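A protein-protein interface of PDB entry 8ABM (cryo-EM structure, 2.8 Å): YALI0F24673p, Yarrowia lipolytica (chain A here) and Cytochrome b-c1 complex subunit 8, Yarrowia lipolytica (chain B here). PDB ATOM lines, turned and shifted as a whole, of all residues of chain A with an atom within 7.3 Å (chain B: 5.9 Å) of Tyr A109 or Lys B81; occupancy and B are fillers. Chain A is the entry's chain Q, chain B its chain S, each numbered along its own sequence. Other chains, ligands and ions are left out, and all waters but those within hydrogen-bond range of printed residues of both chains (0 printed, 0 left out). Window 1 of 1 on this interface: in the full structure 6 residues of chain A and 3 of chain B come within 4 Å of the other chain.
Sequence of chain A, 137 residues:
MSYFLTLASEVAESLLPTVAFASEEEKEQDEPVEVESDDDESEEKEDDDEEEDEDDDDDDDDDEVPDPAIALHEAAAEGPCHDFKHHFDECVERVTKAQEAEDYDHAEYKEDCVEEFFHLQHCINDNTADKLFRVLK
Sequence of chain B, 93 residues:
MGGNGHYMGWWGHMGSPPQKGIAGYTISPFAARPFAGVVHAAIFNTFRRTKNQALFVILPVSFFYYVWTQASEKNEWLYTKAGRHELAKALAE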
ATOM      1  N   CYS A  91      12.310  12.220 -21.790  1.00  0.00           N
ATOM      2  CA  CYS A  91      13.678  12.183 -22.286  1.00  0.00           C
ATOM      3  C   CYS A  91      14.613  11.645 -21.205  1.00  0.00           C
ATOM      4  O   CYS A  91      15.377  10.718 -21.489  1.00  0.00           O
ATOM      5  CB  CYS A  91      14.171  13.542 -22.772  1.00  0.00           C
ATOM      6  SG  CYS A  91      15.862  13.539 -23.441  1.00  0.00           S
ATOM      7  N   ARG A  94      14.432   7.933 -20.669  1.00  0.00           N
ATOM      8  CA  ARG A  94      15.038   7.185 -21.765  1.00  0.00           C
ATOM      9  C   ARG A  94      16.557   7.169 -21.634  1.00  0.00           C
ATOM     10  O   ARG A  94      17.174   6.118 -21.804  1.00  0.00           O
ATOM     11  CB  ARG A  94      14.652   7.738 -23.142  1.00  0.00           C
ATOM     12  CG  ARG A  94      13.181   7.551 -23.484  1.00  0.00           C
ATOM     13  CD  ARG A  94      12.647   8.199 -24.747  1.00  0.00           C
ATOM     14  NE  ARG A  94      12.828   9.646 -24.842  1.00  0.00           N
ATOM     15  CZ  ARG A  94      13.578  10.238 -25.764  1.00  0.00           C
ATOM     16  NH1 ARG A  94      14.197   9.491 -26.663  1.00  0.00           N
ATOM     17  NH2 ARG A  94      13.689  11.556 -25.784  1.00  0.00           N
ATOM     18  N   VAL A  95      17.137   8.336 -21.342  1.00  0.00           N
ATOM     19  CA  VAL A  95      18.581   8.482 -21.390  1.00  0.00           C
ATOM     20  C   VAL A  95      19.214   7.750 -20.211  1.00  0.00           C
ATOM     21  O   VAL A  95      20.200   7.043 -20.402  1.00  0.00           O
ATOM     22  CB  VAL A  95      19.020   9.953 -21.498  1.00  0.00           C
ATOM     23  CG1 VAL A  95      20.514  10.124 -21.275  1.00  0.00           C
ATOM     24  CG2 VAL A  95      18.634  10.521 -22.853  1.00  0.00           C
ATOM     25  N   TYR A 104      27.118   0.923 -23.463  1.00  0.00           N
ATOM     26  CA  TYR A 104      26.658   2.266 -23.768  1.00  0.00           C
ATOM     27  C   TYR A 104      27.862   3.144 -24.109  1.00  0.00           C
ATOM     28  O   TYR A 104      27.761   4.026 -24.960  1.00  0.00           O
ATOM     29  CB  TYR A 104      25.800   2.833 -22.628  1.00  0.00           C
ATOM     30  CG  TYR A 104      25.608   4.330 -22.686  1.00  0.00           C
ATOM     31  CD1 TYR A 104      24.669   4.907 -23.532  1.00  0.00           C
ATOM     32  CD2 TYR A 104      26.406   5.180 -21.931  1.00  0.00           C
ATOM     33  CE1 TYR A 104      24.517   6.286 -23.613  1.00  0.00           C
ATOM     34  CE2 TYR A 104      26.271   6.559 -22.005  1.00  0.00           C
ATOM     35  CZ  TYR A 104      25.320   7.115 -22.845  1.00  0.00           C
ATOM     36  OH  TYR A 104      25.172   8.473 -22.901  1.00  0.00           O
ATOM     37  N   HIS A 106      30.538   2.228 -25.571  1.00  0.00           N
ATOM     38  CA  HIS A 106      30.987   1.856 -26.907  1.00  0.00           C
ATOM     39  C   HIS A 106      29.823   1.926 -27.895  1.00  0.00           C
ATOM     40  O   HIS A 106      29.668   1.049 -28.744  1.00  0.00           O
ATOM     41  CB  HIS A 106      31.692   0.487 -26.902  1.00  0.00           C
ATOM     42  CG  HIS A 106      32.959   0.475 -26.111  1.00  0.00           C
ATOM     43  ND1 HIS A 106      34.098   1.147 -26.518  1.00  0.00           N
ATOM     44  CD2 HIS A 106      33.263  -0.097 -24.925  1.00  0.00           C
ATOM     45  CE1 HIS A 106      35.053   0.974 -25.625  1.00  0.00           C
ATOM     46  NE2 HIS A 106      34.565   0.216 -24.634  1.00  0.00           N
ATOM     47  N   ALA A 107      29.009   2.981 -27.771  1.00  0.00           N
ATOM     48  CA  ALA A 107      27.948   3.251 -28.729  1.00  0.00           C
ATOM     49  C   ALA A 107      28.345   4.436 -29.606  1.00  0.00           C
ATOM     50  O   ALA A 107      29.223   5.224 -29.242  1.00  0.00           O
ATOM     51  CB  ALA A 107      26.622   3.454 -28.026  1.00  0.00           C
ATOM     52  N   GLU A 108      27.705   4.533 -30.775  1.00  0.00           N
ATOM     53  CA  GLU A 108      28.013   5.580 -31.734  1.00  0.00           C
ATOM     54  C   GLU A 108      27.378   6.893 -31.269  1.00  0.00           C
ATOM     55  O   GLU A 108      28.074   7.902 -31.111  1.00  0.00           O
ATOM     56  CB  GLU A 108      27.601   5.130 -33.143  1.00  0.00           C
ATOM     57  CG  GLU A 108      28.208   5.962 -34.271  1.00  0.00           C
ATOM     58  CD  GLU A 108      27.545   7.303 -34.561  1.00  0.00           C
ATOM     59  OE1 GLU A 108      28.246   8.340 -34.501  1.00  0.00           O
ATOM     60  OE2 GLU A 108      26.332   7.309 -34.859  1.00  0.00           O
ATOM     61  N   TYR A 109      26.060   6.849 -31.032  1.00  0.00           N
ATOM     62  CA  TYR A 109      25.278   8.024 -30.677  1.00  0.00           C
ATOM     63  C   TYR A 109      24.824   7.945 -29.220  1.00  0.00           C
ATOM     64  O   TYR A 109      24.066   7.050 -28.850  1.00  0.00           O
ATOM     65  CB  TYR A 109      24.084   8.193 -31.623  1.00  0.00           C
ATOM     66  CG  TYR A 109      23.116   9.277 -31.220  1.00  0.00           C
ATOM     67  CD1 TYR A 109      23.504  10.612 -31.199  1.00  0.00           C
ATOM     68  CD2 TYR A 109      21.815   8.973 -30.846  1.00  0.00           C
ATOM     69  CE1 TYR A 109      22.622  11.617 -30.829  1.00  0.00           C
ATOM     70  CE2 TYR A 109      20.919   9.967 -30.477  1.00  0.00           C
ATOM     71  CZ  TYR A 109      21.325  11.293 -30.465  1.00  0.00           C
ATOM     72  OH  TYR A 109      20.456  12.283 -30.102  1.00  0.00           O
ATOM     73  N   LYS A 110      25.267   8.919 -28.415  1.00  0.00           N
ATOM     74  CA  LYS A 110      24.791   9.086 -27.051  1.00  0.00           C
ATOM     75  C   LYS A 110      23.819  10.265 -26.983  1.00  0.00           C
ATOM     76  O   LYS A 110      24.201  11.413 -27.211  1.00  0.00           O
ATOM     77  CB  LYS A 110      25.981   9.242 -26.100  1.00  0.00           C
ATOM     78  CG  LYS A 110      26.947   8.062 -26.064  1.00  0.00           C
ATOM     79  CD  LYS A 110      28.201   8.368 -25.266  1.00  0.00           C
ATOM     80  CE  LYS A 110      29.115   7.177 -25.060  1.00  0.00           C
ATOM     81  NZ  LYS A 110      29.574   6.589 -26.339  1.00  0.00           N
ATOM     82  N   GLU A 111      22.550   9.955 -26.684  1.00  0.00           N
ATOM     83  CA  GLU A 111      21.480  10.940 -26.599  1.00  0.00           C
ATOM     84  C   GLU A 111      21.643  11.771 -25.324  1.00  0.00           C
ATOM     85  O   GLU A 111      21.960  11.220 -24.269  1.00  0.00           O
ATOM     86  CB  GLU A 111      20.126  10.226 -26.604  1.00  0.00           C
ATOM     87  CG  GLU A 111      18.985  11.114 -27.058  1.00  0.00           C
ATOM     88  CD  GLU A 111      17.551  10.707 -26.772  1.00  0.00           C
ATOM     89  OE1 GLU A 111      16.707  11.618 -26.757  1.00  0.00           O
ATOM     90  OE2 GLU A 111      17.268   9.500 -26.587  1.00  0.00           O
ATOM     91  N   ASP A 112      21.407  13.092 -25.432  1.00  0.00           N
ATOM     92  CA  ASP A 112      21.273  13.979 -24.283  1.00  0.00           C
ATOM     93  C   ASP A 112      19.825  14.454 -24.159  1.00  0.00           C
ATOM     94  O   ASP A 112      18.972  14.065 -24.954  1.00  0.00           O
ATOM     95  CB  ASP A 112      22.238  15.163 -24.378  1.00  0.00           C
ATOM     96  CG  ASP A 112      22.097  15.942 -25.676  1.00  0.00           C
ATOM     97  OD1 ASP A 112      21.215  16.825 -25.755  1.00  0.00           O
ATOM     98  OD2 ASP A 112      22.843  15.618 -26.620  1.00  0.00           O
ATOM     99  N   CYS A 113      19.578  15.330 -23.181  1.00  0.00           N
ATOM    100  CA  CYS A 113      18.258  15.900 -22.992  1.00  0.00           C
ATOM    101  C   CYS A 113      18.297  17.420 -23.062  1.00  0.00           C
ATOM    102  O   CYS A 113      17.372  18.089 -22.602  1.00  0.00           O
ATOM    103  CB  CYS A 113      17.657  15.403 -21.689  1.00  0.00           C
ATOM    104  SG  CYS A 113      17.175  13.666 -21.852  1.00  0.00           S
ATOM    105  N   VAL A 114      19.345  17.935 -23.704  1.00  0.00           N
ATOM    106  CA  VAL A 114      19.571  19.365 -23.711  1.00  0.00           C
ATOM    107  C   VAL A 114      18.466  20.047 -24.506  1.00  0.00           C
ATOM    108  O   VAL A 114      17.939  21.068 -24.071  1.00  0.00           O
ATOM    109  CB  VAL A 114      20.968  19.698 -24.249  1.00  0.00           C
ATOM    110  CG1 VAL A 114      21.118  21.165 -24.609  1.00  0.00           C
ATOM    111  CG2 VAL A 114      22.010  19.296 -23.235  1.00  0.00           C
ATOM    112  N   GLU A 115      18.097  19.447 -25.638  1.00  0.00           N
ATOM    113  CA  GLU A 115      17.087  20.044 -26.495  1.00  0.00           C
ATOM    114  C   GLU A 115      15.792  20.280 -25.722  1.00  0.00           C
ATOM    115  O   GLU A 115      15.222  21.370 -25.759  1.00  0.00           O
ATOM    116  CB  GLU A 115      16.828  19.158 -27.706  1.00  0.00           C
ATOM    117  CG  GLU A 115      17.406  19.726 -28.985  1.00  0.00           C
ATOM    118  CD  GLU A 115      17.360  18.779 -30.173  1.00  0.00           C
ATOM    119  OE1 GLU A 115      16.241  18.426 -30.611  1.00  0.00           O
ATOM    120  OE2 GLU A 115      18.446  18.389 -30.660  1.00  0.00           O
ATOM    121  N   GLU A 116      15.348  19.231 -25.025  1.00  0.00           N
ATOM    122  CA  GLU A 116      14.093  19.246 -24.294  1.00  0.00           C
ATOM    123  C   GLU A 116      14.198  20.208 -23.123  1.00  0.00           C
ATOM    124  O   GLU A 116      13.222  20.864 -22.757  1.00  0.00           O
ATOM    125  CB  GLU A 116      13.761  17.847 -23.775  1.00  0.00           C
ATOM    126  CG  GLU A 116      13.189  16.944 -24.847  1.00  0.00           C
ATOM    127  CD  GLU A 116      14.221  16.280 -25.746  1.00  0.00           C
ATOM    128  OE1 GLU A 116      13.811  15.634 -26.725  1.00  0.00           O
ATOM    129  OE2 GLU A 116      15.433  16.455 -25.485  1.00  0.00           O
ATOM    130  N   TRP B  77      15.778  22.650 -38.321  1.00  0.00           N
ATOM    131  CA  TRP B  77      15.331  21.288 -38.124  1.00  0.00           C
ATOM    132  C   TRP B  77      16.485  20.300 -38.298  1.00  0.00           C
ATOM    133  O   TRP B  77      16.499  19.253 -37.662  1.00  0.00           O
ATOM    134  CB  TRP B  77      14.158  20.987 -39.059  1.00  0.00           C
ATOM    135  CG  TRP B  77      13.660  19.584 -38.936  1.00  0.00           C
ATOM    136  CD1 TRP B  77      12.764  19.109 -38.022  1.00  0.00           C
ATOM    137  CD2 TRP B  77      14.054  18.461 -39.740  1.00  0.00           C
ATOM    138  NE1 TRP B  77      12.558  17.771 -38.209  1.00  0.00           N
ATOM    139  CE2 TRP B  77      13.336  17.344 -39.254  1.00  0.00           C
ATOM    140  CE3 TRP B  77      14.930  18.290 -40.821  1.00  0.00           C
ATOM    141  CZ2 TRP B  77      13.478  16.072 -39.810  1.00  0.00           C
ATOM    142  CZ3 TRP B  77      15.054  17.035 -41.382  1.00  0.00           C
ATOM    143  CH2 TRP B  77      14.336  15.945 -40.880  1.00  0.00           C
ATOM    144  N   TYR B  79      19.463  20.632 -37.327  1.00  0.00           N
ATOM    145  CA  TYR B  79      20.343  20.650 -36.175  1.00  0.00           C
ATOM    146  C   TYR B  79      19.558  20.297 -34.918  1.00  0.00           C
ATOM    147  O   TYR B  79      19.965  20.646 -33.811  1.00  0.00           O
ATOM    148  CB  TYR B  79      21.098  21.978 -36.116  1.00  0.00           C
ATOM    149  CG  TYR B  79      22.207  22.059 -37.133  1.00  0.00           C
ATOM    150  CD1 TYR B  79      23.497  21.661 -36.816  1.00  0.00           C
ATOM    151  CD2 TYR B  79      21.956  22.477 -38.434  1.00  0.00           C
ATOM    152  CE1 TYR B  79      24.515  21.702 -37.757  1.00  0.00           C
ATOM    153  CE2 TYR B  79      22.964  22.532 -39.383  1.00  0.00           C
ATOM    154  CZ  TYR B  79      24.249  22.141 -39.044  1.00  0.00           C
ATOM    155  OH  TYR B  79      25.254  22.183 -39.967  1.00  0.00           O
ATOM    156  N   THR B  80      18.420  19.620 -35.104  1.00  0.00           N
ATOM    157  CA  THR B  80      17.740  18.972 -33.995  1.00  0.00           C
ATOM    158  C   THR B  80      18.116  17.493 -34.001  1.00  0.00           C
ATOM    159  O   THR B  80      18.848  17.052 -34.886  1.00  0.00           O
ATOM    160  CB  THR B  80      16.228  19.231 -34.027  1.00  0.00           C
ATOM    161  OG1 THR B  80      15.672  18.617 -35.193  1.00  0.00           O
ATOM    162  CG2 THR B  80      15.870  20.702 -33.992  1.00  0.00           C
ATOM    163  N   LYS B  81      17.625  16.757 -32.996  1.00  0.00           N
ATOM    164  CA  LYS B  81      17.811  15.320 -32.852  1.00  0.00           C
ATOM    165  C   LYS B  81      17.129  14.589 -34.003  1.00  0.00           C
ATOM    166  O   LYS B  81      17.688  13.652 -34.574  1.00  0.00           O
ATOM    167  CB  LYS B  81      17.141  14.838 -31.565  1.00  0.00           C
ATOM    168  CG  LYS B  81      18.049  14.720 -30.353  1.00  0.00           C
ATOM    169  CD  LYS B  81      17.306  14.162 -29.170  1.00  0.00           C
ATOM    170  CE  LYS B  81      17.633  14.887 -27.885  1.00  0.00           C
ATOM    171  NZ  LYS B  81      16.769  14.420 -26.776  1.00  0.00           N
ATOM    172  N   ALA B  82      15.904  15.032 -34.309  1.00  0.00           N
ATOM    173  CA  ALA B  82      15.060  14.484 -35.358  1.00  0.00           C
ATOM    174  C   ALA B  82      15.726  14.613 -36.729  1.00  0.00           C
ATOM    175  O   ALA B  82      15.485  13.792 -37.614  1.00  0.00           O
ATOM    176  CB  ALA B  82      13.729  15.190 -35.328  1.00  0.00           C
ATOM    177  N   GLY B  83      16.576  15.635 -36.884  1.00  0.00           N
ATOM    178  CA  GLY B  83      17.170  15.960 -38.171  1.00  0.00           C
ATOM    179  C   GLY B  83      18.584  15.408 -38.337  1.00  0.00           C
ATOM    180  O   GLY B  83      19.277  15.811 -39.270  1.00  0.00           O
ATOM    181  N   ARG B  84      18.985  14.488 -37.444  1.00  0.00           N
ATOM    182  CA  ARG B  84      20.342  13.965 -37.364  1.00  0.00           C
ATOM    183  C   ARG B  84      20.743  13.294 -38.670  1.00  0.00           C
ATOM    184  O   ARG B  84      21.870  13.451 -39.139  1.00  0.00           O
ATOM    185  CB  ARG B  84      20.418  12.818 -36.362  1.00  0.00           C
ATOM    186  CG  ARG B  84      20.869  13.234 -34.973  1.00  0.00           C
ATOM    187  CD  ARG B  84      21.251  11.969 -34.238  1.00  0.00           C
ATOM    188  NE  ARG B  84      20.126  11.072 -33.997  1.00  0.00           N
ATOM    189  CZ  ARG B  84      20.165   9.749 -34.134  1.00  0.00           C
ATOM    190  NH1 ARG B  84      21.274   9.149 -34.535  1.00  0.00           N
ATOM    191  NH2 ARG B  84      19.083   9.032 -33.886  1.00  0.00           N
ATOM    192  N   HIS B  85      19.811  12.499 -39.199  1.00  0.00           N
ATOM    193  CA  HIS B  85      20.085  11.629 -40.323  1.00  0.00           C
ATOM    194  C   HIS B  85      20.174  12.453 -41.596  1.00  0.00           C
ATOM    195  O   HIS B  85      21.015  12.188 -42.452  1.00  0.00           O
ATOM    196  CB  HIS B  85      18.984  10.580 -40.458  1.00  0.00           C
ATOM    197  CG  HIS B  85      18.861   9.715 -39.254  1.00  0.00           C
ATOM    198  ND1 HIS B  85      19.872   8.864 -38.848  1.00  0.00           N
ATOM    199  CD2 HIS B  85      17.856   9.566 -38.367  1.00  0.00           C
ATOM    200  CE1 HIS B  85      19.491   8.224 -37.760  1.00  0.00           C
ATOM    201  NE2 HIS B  85      18.255   8.636 -37.448  1.00  0.00           N
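The side-chain sulfur of Cys A91 sits at hydrogen-bond distance from the side-chain amino group of Lys B81 (3.6 Å).
The side-chain carboxylate of Glu A111 is in salt-bridge range of the side-chain amino group of Lys B81.
The backbone carbonyl oxygen of Asp A112 sits at hydrogen-bond distance from the side-chain amino group of Lys B81, 2.9 Å away.
N of Lys B81 lies within hydrogen-bond range of OE2 of Glu A115, at 3.0 Å.
The side-chain carboxylate (OE2) of Glu A116 is in salt-bridge range of the side-chain amino group (NZ) of Lys B81.
NH2 of Arg A94 sits close to SG of Cys A91 (3.8 Å).
SG of Cys A91 is disulfide-bonded to SG of Cys A113.
NH1 of Arg A94 is in salt-bridge range of OE2 of Glu A111 (3.1 Å).
OD1 of Asp A112 sits at hydrogen-bond distance from N of Val A114, 3.0 Å away.
The backbone carbonyl oxygen (O) of Trp B77 sits at hydrogen-bond distance from the side-chain hydroxyl (OG1) of Thr B80 (2.7 Å).
Among the printed residues, merely in contact across the chains: Tyr A109 with Lys B81, Glu A115 with Thr B80 and Tyr A109 with Arg B84.
Of the printed residues of chain B, Cys A91 touches Lys B81 (3.6 Å).
Tyr A104 touches none of the printed residues of chain B.
Of the printed residues of chain B, Tyr A109 touches Lys B81 and Arg B84.
Of the printed residues of chain B, Asp A112 touches Lys B81.
Printed residues of chain B within 4 Å of Glu A116: Lys B81 (2.8 Å).
Lys B81 touches six residues of chain A.
Gly B83 touches none of the printed residues of chain A.
Of the printed residues of chain A, Arg B84 touches Tyr A109.
Hydrophobic or aromatic side chains of chain A within 4 Å of the printed part of chain B: Tyr A109.
Among the printed residues, Asp or Glu carboxylates within 4 Å of a Lys or Arg side-chain nitrogen of the other chain: Glu A111 with Lys B81 (2.8 Å) and Glu A116 with Lys B81 (2.8 Å).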
